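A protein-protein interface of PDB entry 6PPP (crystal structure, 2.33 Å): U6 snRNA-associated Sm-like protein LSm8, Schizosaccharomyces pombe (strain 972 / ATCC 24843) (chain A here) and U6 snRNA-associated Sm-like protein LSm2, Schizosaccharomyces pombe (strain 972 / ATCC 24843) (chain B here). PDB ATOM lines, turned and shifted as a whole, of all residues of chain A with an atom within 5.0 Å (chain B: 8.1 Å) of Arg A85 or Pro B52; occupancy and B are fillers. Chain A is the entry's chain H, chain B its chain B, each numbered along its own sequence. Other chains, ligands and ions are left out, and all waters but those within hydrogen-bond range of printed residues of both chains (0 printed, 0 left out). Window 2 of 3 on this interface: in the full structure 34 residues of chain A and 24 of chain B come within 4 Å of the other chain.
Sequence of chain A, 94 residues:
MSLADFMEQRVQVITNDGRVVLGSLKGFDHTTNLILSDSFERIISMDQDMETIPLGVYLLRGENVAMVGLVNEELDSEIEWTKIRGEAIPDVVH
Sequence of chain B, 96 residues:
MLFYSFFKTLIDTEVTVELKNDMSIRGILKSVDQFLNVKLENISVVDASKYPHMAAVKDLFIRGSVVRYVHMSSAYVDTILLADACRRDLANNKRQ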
ATOM      1  N   ILE A  44     -11.356  25.854  -3.477  1.00  0.00           N
ATOM      2  CA  ILE A  44     -12.569  25.161  -3.090  1.00  0.00           C
ATOM      3  C   ILE A  44     -12.207  23.838  -2.435  1.00  0.00           C
ATOM      4  O   ILE A  44     -11.309  23.125  -2.928  1.00  0.00           O
ATOM      5  CB  ILE A  44     -13.453  24.950  -4.330  1.00  0.00           C
ATOM      6  CG1 ILE A  44     -13.904  26.309  -4.881  1.00  0.00           C
ATOM      7  CG2 ILE A  44     -14.664  24.095  -3.984  1.00  0.00           C
ATOM      8  CD1 ILE A  44     -14.441  26.254  -6.320  1.00  0.00           C
ATOM      9  N   SER A  45     -12.903  23.496  -1.336  1.00  0.00           N
ATOM     10  CA  SER A  45     -12.653  22.275  -0.578  1.00  0.00           C
ATOM     11  C   SER A  45     -13.987  21.640  -0.260  1.00  0.00           C
ATOM     12  O   SER A  45     -15.052  22.170  -0.584  1.00  0.00           O
ATOM     13  CB  SER A  45     -12.118  22.591   0.858  1.00  0.00           C
ATOM     14  OG  SER A  45     -10.828  23.126   0.948  1.00  0.00           O
ATOM     15  N   MET A  46     -13.933  20.468   0.361  1.00  0.00           N
ATOM     16  CA  MET A  46     -15.126  19.878   0.939  1.00  0.00           C
ATOM     17  C   MET A  46     -15.209  20.129   2.429  1.00  0.00           C
ATOM     18  O   MET A  46     -16.316  20.217   2.965  1.00  0.00           O
ATOM     19  CB  MET A  46     -15.183  18.380   0.652  1.00  0.00           C
ATOM     20  CG  MET A  46     -15.439  18.115  -0.795  1.00  0.00           C
ATOM     21  SD  MET A  46     -15.788  16.401  -1.193  1.00  0.00           S
ATOM     22  CE  MET A  46     -14.410  15.564  -0.409  1.00  0.00           C
ATOM     23  N   ASP A  47     -14.046  20.218   3.117  1.00  0.00           N
ATOM     24  CA  ASP A  47     -13.969  20.315   4.576  1.00  0.00           C
ATOM     25  C   ASP A  47     -14.108  21.752   5.066  1.00  0.00           C
ATOM     26  O   ASP A  47     -14.661  21.992   6.151  1.00  0.00           O
ATOM     27  CB  ASP A  47     -12.649  19.714   5.064  1.00  0.00           C
ATOM     28  N   GLN A  48     -13.650  22.711   4.257  1.00  0.00           N
ATOM     29  CA  GLN A  48     -13.575  24.107   4.665  1.00  0.00           C
ATOM     30  C   GLN A  48     -14.105  24.972   3.529  1.00  0.00           C
ATOM     31  O   GLN A  48     -14.132  24.573   2.354  1.00  0.00           O
ATOM     32  CB  GLN A  48     -12.142  24.544   5.050  1.00  0.00           C
ATOM     33  N   ASP A  49     -14.488  26.190   3.906  1.00  0.00           N
ATOM     34  CA  ASP A  49     -14.979  27.195   2.976  1.00  0.00           C
ATOM     35  C   ASP A  49     -13.951  27.543   1.904  1.00  0.00           C
ATOM     36  O   ASP A  49     -12.773  27.177   1.976  1.00  0.00           O
ATOM     37  CB  ASP A  49     -15.422  28.445   3.728  1.00  0.00           C
ATOM     38  CG  ASP A  49     -16.778  28.264   4.397  1.00  0.00           C
ATOM     39  OD1 ASP A  49     -17.458  27.262   4.070  1.00  0.00           O
ATOM     40  OD2 ASP A  49     -17.149  29.108   5.256  1.00  0.00           O
ATOM     41  N   TRP A  81     -20.012  32.051  -3.949  1.00  0.00           N
ATOM     42  CA  TRP A  81     -18.837  31.198  -3.891  1.00  0.00           C
ATOM     43  C   TRP A  81     -18.314  30.981  -2.471  1.00  0.00           C
ATOM     44  O   TRP A  81     -17.619  29.988  -2.234  1.00  0.00           O
ATOM     45  CB  TRP A  81     -17.736  31.813  -4.755  1.00  0.00           C
ATOM     46  CG  TRP A  81     -17.963  31.769  -6.227  1.00  0.00           C
ATOM     47  CD1 TRP A  81     -18.317  32.813  -7.051  1.00  0.00           C
ATOM     48  CD2 TRP A  81     -17.789  30.631  -7.076  1.00  0.00           C
ATOM     49  NE1 TRP A  81     -18.391  32.377  -8.361  1.00  0.00           N
ATOM     50  CE2 TRP A  81     -18.075  31.040  -8.395  1.00  0.00           C
ATOM     51  CE3 TRP A  81     -17.428  29.299  -6.847  1.00  0.00           C
ATOM     52  CZ2 TRP A  81     -18.012  30.161  -9.470  1.00  0.00           C
ATOM     53  CZ3 TRP A  81     -17.360  28.436  -7.917  1.00  0.00           C
ATOM     54  CH2 TRP A  81     -17.653  28.864  -9.204  1.00  0.00           C
ATOM     55  N   LYS A  83     -19.845  30.013   0.408  1.00  0.00           N
ATOM     56  CA  LYS A  83     -20.406  28.778   0.950  1.00  0.00           C
ATOM     57  C   LYS A  83     -20.386  27.608  -0.032  1.00  0.00           C
ATOM     58  O   LYS A  83     -21.229  26.705   0.084  1.00  0.00           O
ATOM     59  CB  LYS A  83     -21.837  29.040   1.424  1.00  0.00           C
ATOM     60  N   ILE A  84     -19.407  27.534  -0.930  1.00  0.00           N
ATOM     61  CA  ILE A  84     -19.355  26.478  -1.936  1.00  0.00           C
ATOM     62  C   ILE A  84     -18.332  25.426  -1.542  1.00  0.00           C
ATOM     63  O   ILE A  84     -17.217  25.748  -1.100  1.00  0.00           O
ATOM     64  CB  ILE A  84     -19.026  27.051  -3.325  1.00  0.00           C
ATOM     65  CG1 ILE A  84     -20.206  27.869  -3.866  1.00  0.00           C
ATOM     66  CG2 ILE A  84     -18.573  25.955  -4.306  1.00  0.00           C
ATOM     67  CD1 ILE A  84     -21.155  27.113  -4.796  1.00  0.00           C
ATOM     68  N   ARG A  85     -18.746  24.164  -1.636  1.00  0.00           N
ATOM     69  CA  ARG A  85     -17.875  23.041  -1.354  1.00  0.00           C
ATOM     70  C   ARG A  85     -17.806  22.147  -2.588  1.00  0.00           C
ATOM     71  O   ARG A  85     -18.770  22.033  -3.355  1.00  0.00           O
ATOM     72  CB  ARG A  85     -18.361  22.257  -0.156  1.00  0.00           C
ATOM     73  CG  ARG A  85     -18.490  23.099   1.097  1.00  0.00           C
ATOM     74  CD  ARG A  85     -17.186  23.797   1.439  1.00  0.00           C
ATOM     75  NE  ARG A  85     -17.225  24.351   2.794  1.00  0.00           N
ATOM     76  CZ  ARG A  85     -17.145  23.629   3.912  1.00  0.00           C
ATOM     77  NH1 ARG A  85     -17.020  22.309   3.859  1.00  0.00           N
ATOM     78  NH2 ARG A  85     -17.193  24.227   5.094  1.00  0.00           N
ATOM     79  N   GLY A  86     -16.665  21.483  -2.748  1.00  0.00           N
ATOM     80  CA  GLY A  86     -16.424  20.635  -3.902  1.00  0.00           C
ATOM     81  C   GLY A  86     -15.142  19.858  -3.709  1.00  0.00           C
ATOM     82  O   GLY A  86     -14.347  20.133  -2.803  1.00  0.00           O
ATOM     83  N   GLU A  87     -14.937  18.897  -4.602  1.00  0.00           N
ATOM     84  CA  GLU A  87     -13.758  18.045  -4.555  1.00  0.00           C
ATOM     85  C   GLU A  87     -12.570  18.742  -5.200  1.00  0.00           C
ATOM     86  O   GLU A  87     -12.736  19.609  -6.055  1.00  0.00           O
ATOM     87  CB  GLU A  87     -14.072  16.697  -5.212  1.00  0.00           C
ATOM     88  CG  GLU A  87     -15.310  16.052  -4.564  1.00  0.00           C
ATOM     89  CD  GLU A  87     -15.379  14.544  -4.694  1.00  0.00           C
ATOM     90  OE1 GLU A  87     -14.377  13.935  -5.133  1.00  0.00           O
ATOM     91  OE2 GLU A  87     -16.435  13.976  -4.321  1.00  0.00           O
ATOM     92  N   VAL B  45     -19.928  20.588 -17.212  1.00  0.00           N
ATOM     93  CA  VAL B  45     -19.047  19.558 -16.671  1.00  0.00           C
ATOM     94  C   VAL B  45     -19.865  18.328 -16.325  1.00  0.00           C
ATOM     95  O   VAL B  45     -20.892  18.437 -15.637  1.00  0.00           O
ATOM     96  CB  VAL B  45     -18.295  20.131 -15.460  1.00  0.00           C
ATOM     97  CG1 VAL B  45     -17.146  19.260 -15.074  1.00  0.00           C
ATOM     98  CG2 VAL B  45     -17.792  21.557 -15.768  1.00  0.00           C
ATOM     99  N   ASP B  47     -19.637  15.759 -14.199  1.00  0.00           N
ATOM    100  CA  ASP B  47     -19.964  15.443 -12.816  1.00  0.00           C
ATOM    101  C   ASP B  47     -19.974  16.733 -12.013  1.00  0.00           C
ATOM    102  O   ASP B  47     -19.088  16.999 -11.189  1.00  0.00           O
ATOM    103  CB  ASP B  47     -18.996  14.447 -12.277  1.00  0.00           C
ATOM    104  CG  ASP B  47     -19.514  13.742 -11.089  1.00  0.00           C
ATOM    105  OD1 ASP B  47     -20.344  14.341 -10.361  1.00  0.00           O
ATOM    106  OD2 ASP B  47     -19.060  12.595 -10.873  1.00  0.00           O
ATOM    107  N   ALA B  48     -21.006  17.535 -12.248  1.00  0.00           N
ATOM    108  CA  ALA B  48     -20.935  18.923 -11.834  1.00  0.00           C
ATOM    109  C   ALA B  48     -20.933  19.037 -10.322  1.00  0.00           C
ATOM    110  O   ALA B  48     -20.377  20.004  -9.794  1.00  0.00           O
ATOM    111  CB  ALA B  48     -22.085  19.728 -12.417  1.00  0.00           C
ATOM    112  N   SER B  49     -21.492  18.058  -9.606  1.00  0.00           N
ATOM    113  CA  SER B  49     -21.457  18.125  -8.149  1.00  0.00           C
ATOM    114  C   SER B  49     -20.078  17.845  -7.578  1.00  0.00           C
ATOM    115  O   SER B  49     -19.755  18.337  -6.486  1.00  0.00           O
ATOM    116  CB  SER B  49     -22.402  17.026  -7.604  1.00  0.00           C
ATOM    117  OG  SER B  49     -21.758  15.750  -7.648  1.00  0.00           O
ATOM    118  N   LYS B  50     -19.260  17.038  -8.265  1.00  0.00           N
ATOM    119  CA  LYS B  50     -17.868  16.941  -7.850  1.00  0.00           C
ATOM    120  C   LYS B  50     -17.160  18.267  -8.057  1.00  0.00           C
ATOM    121  O   LYS B  50     -16.462  18.768  -7.169  1.00  0.00           O
ATOM    122  CB  LYS B  50     -17.142  15.859  -8.659  1.00  0.00           C
ATOM    123  CG  LYS B  50     -17.747  14.480  -8.527  1.00  0.00           C
ATOM    124  CD  LYS B  50     -16.728  13.413  -8.903  1.00  0.00           C
ATOM    125  CE  LYS B  50     -15.586  13.435  -7.884  1.00  0.00           C
ATOM    126  NZ  LYS B  50     -14.904  12.123  -7.632  1.00  0.00           N
ATOM    127  N   TYR B  51     -17.424  18.890  -9.200  1.00  0.00           N
ATOM    128  CA  TYR B  51     -16.696  20.062  -9.661  1.00  0.00           C
ATOM    129  C   TYR B  51     -17.547  21.290  -9.960  1.00  0.00           C
ATOM    130  O   TYR B  51     -17.923  21.520 -11.120  1.00  0.00           O
ATOM    131  CB  TYR B  51     -15.956  19.668 -10.934  1.00  0.00           C
ATOM    132  CG  TYR B  51     -15.115  18.408 -10.848  1.00  0.00           C
ATOM    133  CD1 TYR B  51     -14.061  18.298  -9.941  1.00  0.00           C
ATOM    134  CD2 TYR B  51     -15.348  17.340 -11.711  1.00  0.00           C
ATOM    135  CE1 TYR B  51     -13.259  17.146  -9.900  1.00  0.00           C
ATOM    136  CE2 TYR B  51     -14.555  16.184 -11.679  1.00  0.00           C
ATOM    137  CZ  TYR B  51     -13.512  16.104 -10.778  1.00  0.00           C
ATOM    138  OH  TYR B  51     -12.737  14.967 -10.752  1.00  0.00           O
ATOM    139  N   PRO B  52     -17.934  22.055  -8.935  1.00  0.00           N
ATOM    140  CA  PRO B  52     -18.679  23.301  -9.160  1.00  0.00           C
ATOM    141  C   PRO B  52     -17.796  24.459  -9.623  1.00  0.00           C
ATOM    142  O   PRO B  52     -18.319  25.569  -9.806  1.00  0.00           O
ATOM    143  CB  PRO B  52     -19.287  23.589  -7.796  1.00  0.00           C
ATOM    144  CG  PRO B  52     -18.291  23.019  -6.846  1.00  0.00           C
ATOM    145  CD  PRO B  52     -17.692  21.804  -7.505  1.00  0.00           C
ATOM    146  N   HIS B  53     -16.478  24.237  -9.844  1.00  0.00           N
ATOM    147  CA  HIS B  53     -15.560  25.353 -10.095  1.00  0.00           C
ATOM    148  C   HIS B  53     -15.927  26.071 -11.370  1.00  0.00           C
ATOM    149  O   HIS B  53     -15.696  27.282 -11.508  1.00  0.00           O
ATOM    150  CB  HIS B  53     -14.101  24.887 -10.276  1.00  0.00           C
ATOM    151  CG  HIS B  53     -13.627  23.859  -9.295  1.00  0.00           C
ATOM    152  ND1 HIS B  53     -14.042  22.542  -9.329  1.00  0.00           N
ATOM    153  CD2 HIS B  53     -12.711  23.941  -8.300  1.00  0.00           C
ATOM    154  CE1 HIS B  53     -13.431  21.869  -8.371  1.00  0.00           C
ATOM    155  NE2 HIS B  53     -12.619  22.693  -7.732  1.00  0.00           N
ATOM    156  N   MET B  54     -16.579  25.370 -12.269  1.00  0.00           N
ATOM    157  CA  MET B  54     -16.844  25.907 -13.583  1.00  0.00           C
ATOM    158  C   MET B  54     -18.313  26.246 -13.706  1.00  0.00           C
ATOM    159  O   MET B  54     -18.867  26.269 -14.810  1.00  0.00           O
ATOM    160  CB  MET B  54     -16.407  24.896 -14.636  1.00  0.00           C
ATOM    161  CG  MET B  54     -14.967  24.442 -14.422  1.00  0.00           C
ATOM    162  SD  MET B  54     -14.155  24.541 -16.028  1.00  0.00           S
ATOM    163  CE  MET B  54     -13.652  26.269 -16.065  1.00  0.00           C
ATOM    164  N   ALA B  55     -18.950  26.508 -12.557  1.00  0.00           N
ATOM    165  CA  ALA B  55     -20.365  26.838 -12.563  1.00  0.00           C
ATOM    166  C   ALA B  55     -20.676  28.138 -13.274  1.00  0.00           C
ATOM    167  O   ALA B  55     -21.791  28.294 -13.780  1.00  0.00           O
ATOM    168  CB  ALA B  55     -20.866  26.962 -11.123  1.00  0.00           C
ATOM    169  N   ALA B  56     -19.695  29.017 -13.438  1.00  0.00           N
ATOM    170  CA  ALA B  56     -19.910  30.295 -14.096  1.00  0.00           C
ATOM    171  C   ALA B  56     -19.286  30.374 -15.479  1.00  0.00           C
ATOM    172  O   ALA B  56     -19.351  31.438 -16.110  1.00  0.00           O
ATOM    173  CB  ALA B  56     -19.366  31.411 -13.211  1.00  0.00           C
ATOM    174  N   VAL B  57     -18.751  29.268 -15.996  1.00  0.00           N
ATOM    175  CA  VAL B  57     -18.078  29.244 -17.293  1.00  0.00           C
ATOM    176  C   VAL B  57     -19.011  28.627 -18.326  1.00  0.00           C
ATOM    177  O   VAL B  57     -19.407  27.457 -18.206  1.00  0.00           O
ATOM    178  CB  VAL B  57     -16.769  28.445 -17.194  1.00  0.00           C
ATOM    179  CG1 VAL B  57     -16.342  27.927 -18.541  1.00  0.00           C
ATOM    180  CG2 VAL B  57     -15.693  29.296 -16.594  1.00  0.00           C
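Printed residues of chain B that touch a printed residue of chain A: Lys B50, Pro B52 and His B53. Hydrophobic or aromatic side chains of chain B that line the printed part of chain A: Pro B52 and His B53. Of the 12 printed residues of chain A, 6 touch a printed residue of chain B. Hydrophobic or aromatic side chains of chain A within 4 Å of the printed part of chain B: Ile A44, Trp A81 and Ile A84. Among the printed residues, 9 pairs touch across the chains. Among the printed residues, Asp or Glu carboxylates within 4 Å of a Lys or Arg side-chain nitrogen of the other chain: Glu A87 with Lys B50 (3.1 Å).
Printed residues of chain B within 4 Å of Ile A44: His B53. Of the printed residues of chain B, Trp A81 touches Pro B52 (3.4 Å) and His B53 (3.4 Å). Of the printed residues of chain B, Ile A84 touches Pro B52 (3.9 Å). Arg A85 touches just one residue of chain B: Pro B52 (3.7 Å). Of the printed residues of chain B, Glu A87 touches Lys B50 and His B53. Of the printed residues of chain A, Pro B52 touches Trp A81, Ile A84, Arg A85 and Gly A86. Of the printed residues of chain A, His B53 touches Ile A44 (3.5 Å), Trp A81 (3.4 Å) and Glu A87 (3.3 Å). The nearest printed residue of chain A that does not touch Pro B52 is Ile A44 (4.7 Å).
The backbone NH (N) of Met A46 lies close to the backbone carbonyl oxygen (O) of Gly A86, 3.2 Å away. The guanidinium group (NE) of Arg A85 is in salt-bridge range of the side-chain carboxylate (OD1) of Asp A49 (3.2 Å). The backbone carbonyl oxygen (O) of Gln A48 is in hydrogen-bond range of the guanidinium group (NE) of Arg A85 (3.1 Å). The backbone carbonyl oxygen (O) of Asp A47 lies close to the guanidinium group (NH1) of Arg A85, 3.3 Å away. The backbone NH of Gly A86 sits at hydrogen-bond distance from the backbone carbonyl oxygen of Ser A45 (2.8 Å).
Ile A44 touches His B53. O of Pro B52 touches CH2 of Trp A81, at 3.4 Å. His B53 touches Trp A81 (O to CH2, 3.4 Å). CG2 of Ile A84 touches CG of Pro B52 (3.9 Å). Pro B52 touches Arg A85 (CG to O, 3.7 Å). O of Lys B50 touches CA of Gly A86, 3.8 Å away. CD of Pro B52 touches CA of Gly A86, at 3.99 Å. His B53 touches Glu A87.
NZ of Lys B50 is in salt-bridge range of OE1 of Glu A87, at 3.1 Å.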
